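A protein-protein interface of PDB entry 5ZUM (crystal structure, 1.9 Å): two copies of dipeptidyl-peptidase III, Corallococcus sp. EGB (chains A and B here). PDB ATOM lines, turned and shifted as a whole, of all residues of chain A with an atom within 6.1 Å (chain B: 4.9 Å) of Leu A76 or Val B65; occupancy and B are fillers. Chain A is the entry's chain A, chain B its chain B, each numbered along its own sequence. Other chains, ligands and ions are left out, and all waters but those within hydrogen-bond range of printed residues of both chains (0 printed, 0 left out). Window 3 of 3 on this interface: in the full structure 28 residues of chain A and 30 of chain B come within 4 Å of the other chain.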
ATOM      1  N   LEU A   8     -24.054  -4.166  -5.018  1.00  0.00           N
ATOM      2  CA  LEU A   8     -22.902  -5.055  -5.108  1.00  0.00           C
ATOM      3  C   LEU A   8     -23.101  -6.281  -4.228  1.00  0.00           C
ATOM      4  O   LEU A   8     -22.833  -7.398  -4.657  1.00  0.00           O
ATOM      5  CB  LEU A   8     -21.603  -4.314  -4.775  1.00  0.00           C
ATOM      6  CG  LEU A   8     -20.326  -5.137  -4.833  1.00  0.00           C
ATOM      7  CD1 LEU A   8     -20.133  -5.742  -6.222  1.00  0.00           C
ATOM      8  CD2 LEU A   8     -19.145  -4.265  -4.424  1.00  0.00           C
ATOM      9  N   LEU A  61      -5.695  -4.837  -3.209  1.00  0.00           N
ATOM     10  CA  LEU A  61      -6.131  -5.547  -2.016  1.00  0.00           C
ATOM     11  C   LEU A  61      -5.807  -4.729  -0.752  1.00  0.00           C
ATOM     12  O   LEU A  61      -6.641  -4.607   0.137  1.00  0.00           O
ATOM     13  CB  LEU A  61      -5.486  -6.925  -1.916  1.00  0.00           C
ATOM     14  CG  LEU A  61      -5.698  -7.691  -0.606  1.00  0.00           C
ATOM     15  CD1 LEU A  61      -7.181  -7.826  -0.300  1.00  0.00           C
ATOM     16  CD2 LEU A  61      -4.999  -9.037  -0.651  1.00  0.00           C
ATOM     17  N   LEU A  64      -8.375  -2.043  -0.408  1.00  0.00           N
ATOM     18  CA  LEU A  64      -9.679  -2.569  -0.020  1.00  0.00           C
ATOM     19  C   LEU A  64      -9.754  -3.011   1.442  1.00  0.00           C
ATOM     20  O   LEU A  64     -10.831  -3.008   2.052  1.00  0.00           O
ATOM     21  CB  LEU A  64     -10.066  -3.727  -0.931  1.00  0.00           C
ATOM     22  CG  LEU A  64     -10.229  -3.435  -2.416  1.00  0.00           C
ATOM     23  CD1 LEU A  64     -10.549  -4.737  -3.118  1.00  0.00           C
ATOM     24  CD2 LEU A  64     -11.306  -2.408  -2.731  1.00  0.00           C
ATOM     25  N   VAL A  65      -8.636  -3.458   1.993  1.00  0.00           N
ATOM     26  CA  VAL A  65      -8.575  -3.878   3.376  1.00  0.00           C
ATOM     27  C   VAL A  65      -8.709  -2.681   4.322  1.00  0.00           C
ATOM     28  O   VAL A  65      -9.021  -2.848   5.505  1.00  0.00           O
ATOM     29  CB  VAL A  65      -7.272  -4.660   3.611  1.00  0.00           C
ATOM     30  CG1 VAL A  65      -6.863  -4.652   5.064  1.00  0.00           C
ATOM     31  CG2 VAL A  65      -7.418  -6.097   3.105  1.00  0.00           C
ATOM     32  N   ASP A  67     -10.762   0.200   3.535  1.00  0.00           N
ATOM     33  CA  ASP A  67     -12.125   0.721   3.502  1.00  0.00           C
ATOM     34  C   ASP A  67     -13.082  -0.216   4.233  1.00  0.00           C
ATOM     35  O   ASP A  67     -13.437  -1.272   3.713  1.00  0.00           O
ATOM     36  CB  ASP A  67     -12.563   0.915   2.053  1.00  0.00           C
ATOM     37  CG  ASP A  67     -13.906   1.608   1.922  1.00  0.00           C
ATOM     38  OD1 ASP A  67     -14.633   1.772   2.932  1.00  0.00           O
ATOM     39  OD2 ASP A  67     -14.255   1.947   0.770  1.00  0.00           O
ATOM     40  N   LEU A  71     -19.762  -0.230   1.865  1.00  0.00           N
ATOM     41  CA  LEU A  71     -19.300  -0.334   0.486  1.00  0.00           C
ATOM     42  C   LEU A  71     -17.962  -1.010   0.422  1.00  0.00           C
ATOM     43  O   LEU A  71     -17.750  -1.908  -0.388  1.00  0.00           O
ATOM     44  CB  LEU A  71     -19.176   1.038  -0.168  1.00  0.00           C
ATOM     45  CG  LEU A  71     -18.768   1.005  -1.650  1.00  0.00           C
ATOM     46  CD1 LEU A  71     -19.734   0.158  -2.458  1.00  0.00           C
ATOM     47  CD2 LEU A  71     -18.701   2.409  -2.202  1.00  0.00           C
ATOM     48  N   GLY A  72     -17.059  -0.554   1.278  1.00  0.00           N
ATOM     49  CA  GLY A  72     -15.762  -1.170   1.406  1.00  0.00           C
ATOM     50  C   GLY A  72     -15.860  -2.658   1.623  1.00  0.00           C
ATOM     51  O   GLY A  72     -15.184  -3.438   0.949  1.00  0.00           O
ATOM     52  N   LYS A  73     -16.673  -3.057   2.588  1.00  0.00           N
ATOM     53  CA  LYS A  73     -16.760  -4.452   2.964  1.00  0.00           C
ATOM     54  C   LYS A  73     -17.301  -5.284   1.796  1.00  0.00           C
ATOM     55  O   LYS A  73     -16.837  -6.396   1.579  1.00  0.00           O
ATOM     56  CB  LYS A  73     -17.603  -4.625   4.222  1.00  0.00           C
ATOM     57  CG  LYS A  73     -16.863  -4.273   5.506  1.00  0.00           C
ATOM     58  CD  LYS A  73     -17.778  -4.174   6.708  1.00  0.00           C
ATOM     59  CE  LYS A  73     -16.933  -3.743   7.888  1.00  0.00           C
ATOM     60  NZ  LYS A  73     -17.712  -3.600   9.144  1.00  0.00           N
ATOM     61  N   GLU A  74     -18.268  -4.749   1.054  1.00  0.00           N
ATOM     62  CA  GLU A  74     -18.843  -5.460  -0.087  1.00  0.00           C
ATOM     63  C   GLU A  74     -17.829  -5.488  -1.214  1.00  0.00           C
ATOM     64  O   GLU A  74     -17.772  -6.466  -1.939  1.00  0.00           O
ATOM     65  CB  GLU A  74     -20.121  -4.812  -0.622  1.00  0.00           C
ATOM     66  CG  GLU A  74     -21.323  -4.894   0.312  1.00  0.00           C
ATOM     67  CD  GLU A  74     -21.559  -6.302   0.812  1.00  0.00           C
ATOM     68  OE1 GLU A  74     -21.486  -7.252  -0.009  1.00  0.00           O
ATOM     69  OE2 GLU A  74     -21.792  -6.463   2.018  1.00  0.00           O
ATOM     70  N   ARG A  75     -17.073  -4.404  -1.384  1.00  0.00           N
ATOM     71  CA  ARG A  75     -15.997  -4.406  -2.350  1.00  0.00           C
ATOM     72  C   ARG A  75     -14.937  -5.457  -2.047  1.00  0.00           C
ATOM     73  O   ARG A  75     -14.512  -6.177  -2.945  1.00  0.00           O
ATOM     74  CB  ARG A  75     -15.383  -3.019  -2.487  1.00  0.00           C
ATOM     75  CG  ARG A  75     -16.209  -2.104  -3.373  1.00  0.00           C
ATOM     76  CD  ARG A  75     -15.683  -0.672  -3.351  1.00  0.00           C
ATOM     77  NE  ARG A  75     -16.418   0.132  -4.316  1.00  0.00           N
ATOM     78  CZ  ARG A  75     -16.211   1.427  -4.528  1.00  0.00           C
ATOM     79  NH1 ARG A  75     -15.249   2.075  -3.886  1.00  0.00           N
ATOM     80  NH2 ARG A  75     -16.960   2.067  -5.405  1.00  0.00           N
ATOM     81  N   LEU A  76     -14.577  -5.626  -0.784  1.00  0.00           N
ATOM     82  CA  LEU A  76     -13.585  -6.622  -0.431  1.00  0.00           C
ATOM     83  C   LEU A  76     -14.085  -8.035  -0.688  1.00  0.00           C
ATOM     84  O   LEU A  76     -13.399  -8.849  -1.278  1.00  0.00           O
ATOM     85  CB  LEU A  76     -13.162  -6.454   1.012  1.00  0.00           C
ATOM     86  CG  LEU A  76     -12.222  -7.518   1.531  1.00  0.00           C
ATOM     87  CD1 LEU A  76     -10.930  -7.505   0.730  1.00  0.00           C
ATOM     88  CD2 LEU A  76     -12.012  -7.300   3.002  1.00  0.00           C
ATOM     89  N   HIS A  77     -15.282  -8.319  -0.241  1.00  0.00           N
ATOM     90  CA  HIS A  77     -15.863  -9.620  -0.446  1.00  0.00           C
ATOM     91  C   HIS A  77     -15.927  -9.979  -1.945  1.00  0.00           C
ATOM     92  O   HIS A  77     -15.505 -11.024  -2.337  1.00  0.00           O
ATOM     93  CB  HIS A  77     -17.251  -9.630   0.166  1.00  0.00           C
ATOM     94  CG  HIS A  77     -17.896 -10.962   0.161  1.00  0.00           C
ATOM     95  ND1 HIS A  77     -19.228 -11.137   0.416  1.00  0.00           N
ATOM     96  CD2 HIS A  77     -17.391 -12.188  -0.063  1.00  0.00           C
ATOM     97  CE1 HIS A  77     -19.524 -12.410   0.326  1.00  0.00           C
ATOM     98  NE2 HIS A  77     -18.423 -13.072   0.059  1.00  0.00           N
ATOM     99  N   ALA A  78     -16.448  -9.079  -2.748  1.00  0.00           N
ATOM    100  CA  ALA A  78     -16.529  -9.296  -4.194  1.00  0.00           C
ATOM    101  C   ALA A  78     -15.159  -9.456  -4.839  1.00  0.00           C
ATOM    102  O   ALA A  78     -15.008 -10.260  -5.754  1.00  0.00           O
ATOM    103  CB  ALA A  78     -17.298  -8.170  -4.858  1.00  0.00           C
ATOM    104  N   PHE A  79     -14.182  -8.669  -4.388  1.00  0.00           N
ATOM    105  CA  PHE A  79     -12.802  -8.787  -4.881  1.00  0.00           C
ATOM    106  C   PHE A  79     -12.264 -10.187  -4.620  1.00  0.00           C
ATOM    107  O   PHE A  79     -11.714 -10.830  -5.510  1.00  0.00           O
ATOM    108  CB  PHE A  79     -11.914  -7.722  -4.204  1.00  0.00           C
ATOM    109  CG  PHE A  79     -10.441  -7.828  -4.544  1.00  0.00           C
ATOM    110  CD1 PHE A  79      -9.925  -7.220  -5.694  1.00  0.00           C
ATOM    111  CD2 PHE A  79      -9.604  -8.618  -3.771  1.00  0.00           C
ATOM    112  CE1 PHE A  79      -8.581  -7.333  -5.998  1.00  0.00           C
ATOM    113  CE2 PHE A  79      -8.268  -8.783  -4.107  1.00  0.00           C
ATOM    114  CZ  PHE A  79      -7.756  -8.138  -5.217  1.00  0.00           C
ATOM    115  N   LEU A  80     -12.441 -10.681  -3.401  1.00  0.00           N
ATOM    116  CA  LEU A  80     -11.949 -12.004  -3.051  1.00  0.00           C
ATOM    117  C   LEU A  80     -12.707 -13.115  -3.786  1.00  0.00           C
ATOM    118  O   LEU A  80     -12.095 -14.000  -4.385  1.00  0.00           O
ATOM    119  CB  LEU A  80     -11.956 -12.223  -1.550  1.00  0.00           C
ATOM    120  CG  LEU A  80     -10.994 -11.347  -0.730  1.00  0.00           C
ATOM    121  CD1 LEU A  80     -11.266 -11.445   0.754  1.00  0.00           C
ATOM    122  CD2 LEU A  80      -9.525 -11.681  -0.977  1.00  0.00           C
ATOM    123  N   LEU A  81     -14.030 -13.024  -3.840  1.00  0.00           N
ATOM    124  CA  LEU A  81     -14.814 -13.994  -4.594  1.00  0.00           C
ATOM    125  C   LEU A  81     -14.478 -14.077  -6.083  1.00  0.00           C
ATOM    126  O   LEU A  81     -14.541 -15.171  -6.657  1.00  0.00           O
ATOM    127  CB  LEU A  81     -16.312 -13.773  -4.398  1.00  0.00           C
ATOM    128  CG  LEU A  81     -17.217 -14.907  -4.906  1.00  0.00           C
ATOM    129  CD1 LEU A  81     -18.470 -14.989  -4.034  1.00  0.00           C
ATOM    130  CD2 LEU A  81     -17.602 -14.718  -6.373  1.00  0.00           C
ATOM    131  N   ILE A  96     -15.049  -1.838  -9.217  1.00  0.00           N
ATOM    132  CA  ILE A  96     -14.146  -0.985  -8.442  1.00  0.00           C
ATOM    133  C   ILE A  96     -13.792   0.196  -9.357  1.00  0.00           C
ATOM    134  O   ILE A  96     -13.607   0.015 -10.570  1.00  0.00           O
ATOM    135  CB  ILE A  96     -12.864  -1.740  -8.082  1.00  0.00           C
ATOM    136  CG1 ILE A  96     -13.179  -3.043  -7.339  1.00  0.00           C
ATOM    137  CG2 ILE A  96     -11.881  -0.886  -7.283  1.00  0.00           C
ATOM    138  CD1 ILE A  96     -13.693  -2.885  -5.937  1.00  0.00           C
ATOM    139  N   LEU B  61      -1.744 -12.128   4.980  1.00  0.00           N
ATOM    140  CA  LEU B  61      -2.653 -10.989   4.945  1.00  0.00           C
ATOM    141  C   LEU B  61      -4.091 -11.489   4.709  1.00  0.00           C
ATOM    142  O   LEU B  61      -5.032 -11.104   5.418  1.00  0.00           O
ATOM    143  CB  LEU B  61      -2.222 -10.026   3.851  1.00  0.00           C
ATOM    144  CG  LEU B  61      -3.219  -8.893   3.546  1.00  0.00           C
ATOM    145  CD1 LEU B  61      -3.550  -8.080   4.794  1.00  0.00           C
ATOM    146  CD2 LEU B  61      -2.652  -8.027   2.457  1.00  0.00           C
ATOM    147  N   LEU B  62      -4.226 -12.455   3.805  1.00  0.00           N
ATOM    148  CA  LEU B  62      -5.521 -13.030   3.496  1.00  0.00           C
ATOM    149  C   LEU B  62      -6.113 -13.748   4.681  1.00  0.00           C
ATOM    150  O   LEU B  62      -7.326 -13.723   4.887  1.00  0.00           O
ATOM    151  CB  LEU B  62      -5.410 -13.977   2.308  1.00  0.00           C
ATOM    152  CG  LEU B  62      -5.116 -13.284   0.996  1.00  0.00           C
ATOM    153  CD1 LEU B  62      -4.966 -14.360  -0.069  1.00  0.00           C
ATOM    154  CD2 LEU B  62      -6.254 -12.351   0.619  1.00  0.00           C
ATOM    155  N   ASP B  63      -5.264 -14.356   5.487  1.00  0.00           N
ATOM    156  CA  ASP B  63      -5.715 -14.969   6.735  1.00  0.00           C
ATOM    157  C   ASP B  63      -6.130 -13.862   7.733  1.00  0.00           C
ATOM    158  O   ASP B  63      -7.189 -13.929   8.360  1.00  0.00           O
ATOM    159  CB  ASP B  63      -4.619 -15.863   7.309  1.00  0.00           C
ATOM    160  CG  ASP B  63      -5.144 -16.888   8.304  1.00  0.00           C
ATOM    161  OD1 ASP B  63      -6.209 -17.495   8.044  1.00  0.00           O
ATOM    162  OD2 ASP B  63      -4.463 -17.118   9.334  1.00  0.00           O
ATOM    163  N   LEU B  64      -5.327 -12.812   7.828  1.00  0.00           N
ATOM    164  CA  LEU B  64      -5.586 -11.770   8.833  1.00  0.00           C
ATOM    165  C   LEU B  64      -6.881 -11.024   8.591  1.00  0.00           C
ATOM    166  O   LEU B  64      -7.604 -10.669   9.525  1.00  0.00           O
ATOM    167  CB  LEU B  64      -4.423 -10.786   8.896  1.00  0.00           C
ATOM    168  CG  LEU B  64      -3.182 -11.442   9.508  1.00  0.00           C
ATOM    169  CD1 LEU B  64      -2.105 -10.398   9.756  1.00  0.00           C
ATOM    170  CD2 LEU B  64      -3.474 -12.224  10.776  1.00  0.00           C
ATOM    171  N   VAL B  65      -7.143 -10.738   7.338  1.00  0.00           N
ATOM    172  CA  VAL B  65      -8.310  -9.978   6.970  1.00  0.00           C
ATOM    173  C   VAL B  65      -9.645 -10.681   7.298  1.00  0.00           C
ATOM    174  O   VAL B  65     -10.625 -10.003   7.596  1.00  0.00           O
ATOM    175  CB  VAL B  65      -8.246  -9.597   5.487  1.00  0.00           C
ATOM    176  CG1 VAL B  65      -9.547  -8.974   5.040  1.00  0.00           C
ATOM    177  CG2 VAL B  65      -7.104  -8.633   5.252  1.00  0.00           C
ATOM    178  N   GLU B  66      -9.677 -12.009   7.359  1.00  0.00           N
ATOM    179  CA  GLU B  66     -10.923 -12.744   7.682  1.00  0.00           C
ATOM    180  C   GLU B  66     -11.298 -12.676   9.151  1.00  0.00           C
ATOM    181  O   GLU B  66     -12.418 -13.016   9.522  1.00  0.00           O
ATOM    182  CB  GLU B  66     -10.794 -14.234   7.328  1.00  0.00           C
ATOM    183  CG  GLU B  66     -10.894 -14.536   5.841  1.00  0.00           C
ATOM    184  CD  GLU B  66     -12.217 -14.093   5.251  1.00  0.00           C
ATOM    185  OE1 GLU B  66     -13.258 -14.267   5.926  1.00  0.00           O
ATOM    186  OE2 GLU B  66     -12.202 -13.537   4.136  1.00  0.00           O
ATOM    187  N   ASP B  67     -10.326 -12.353   9.995  1.00  0.00           N
ATOM    188  CA  ASP B  67     -10.558 -12.323  11.418  1.00  0.00           C
ATOM    189  C   ASP B  67     -10.882 -10.887  11.838  1.00  0.00           C
ATOM    190  O   ASP B  67      -9.985 -10.038  11.936  1.00  0.00           O
ATOM    191  CB  ASP B  67      -9.342 -12.873  12.155  1.00  0.00           C
ATOM    192  CG  ASP B  67      -9.561 -12.932  13.636  1.00  0.00           C
ATOM    193  OD1 ASP B  67     -10.670 -12.546  14.043  1.00  0.00           O
ATOM    194  OD2 ASP B  67      -8.648 -13.316  14.404  1.00  0.00           O
ATOM    195  N   THR B  68     -12.185 -10.607  11.943  1.00  0.00           N
ATOM    196  CA  THR B  68     -12.720  -9.286  12.292  1.00  0.00           C
ATOM    197  C   THR B  68     -13.080  -9.194  13.770  1.00  0.00           C
ATOM    198  O   THR B  68     -13.737  -8.257  14.200  1.00  0.00           O
ATOM    199  CB  THR B  68     -13.963  -8.942  11.459  1.00  0.00           C
ATOM    200  OG1 THR B  68     -15.007  -9.880  11.753  1.00  0.00           O
ATOM    201  CG2 THR B  68     -13.643  -8.971   9.963  1.00  0.00           C
ATOM    202  N   LEU B  76      -4.253  -7.131  12.260  1.00  0.00           N
ATOM    203  CA  LEU B  76      -4.174  -6.608  10.936  1.00  0.00           C
ATOM    204  C   LEU B  76      -3.450  -5.254  10.967  1.00  0.00           C
ATOM    205  O   LEU B  76      -2.606  -5.005  10.181  1.00  0.00           O
ATOM    206  CB  LEU B  76      -5.560  -6.445  10.354  1.00  0.00           C
ATOM    207  CG  LEU B  76      -5.670  -5.930   8.928  1.00  0.00           C
ATOM    208  CD1 LEU B  76      -4.822  -6.680   7.930  1.00  0.00           C
ATOM    209  CD2 LEU B  76      -7.102  -5.854   8.483  1.00  0.00           C
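Hydrophobic or aromatic side chains of chain B that line the printed part of chain A: Leu B62, Val B65 and Leu B76. Hydrophobic or aromatic side chains of chain A within 4 Å of the printed part of chain B: Leu A61, Val A65, Leu A76 and Leu A80. Along chain A the printed residues that touch a printed residue of chain B span positions 61 to 80. Among the printed residues, 5 pairs touch across the chains.
Val B65 touches its own counterpart, Val A65. Val A65 touches Leu B76, and with the chains exchanged Leu A76 touches Val B65.
Among the printed residues, merely in contact across the chains: Leu A61 with Leu B62, Val A65 with Val B65, Val A65 with Leu B76, Leu A76 with Val B65 and Leu A80 with Leu B62.
Of chain B, only Val B65 comes within 4 Å of Leu A76. Val B65 touches just these residues of chain A: Val A65 (3.3 Å) and Leu A76 (3.6 Å). Of the printed residues of chain A, Leu B62 touches Leu A61 and Leu A80. Of the printed residues of chain B, Leu A61 touches Leu B62 (3.8 Å). Thr B68 touches none of the printed residues of chain A. The nearest printed residue of chain B that does not touch Leu A80 is Glu B66 (4.1 Å).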
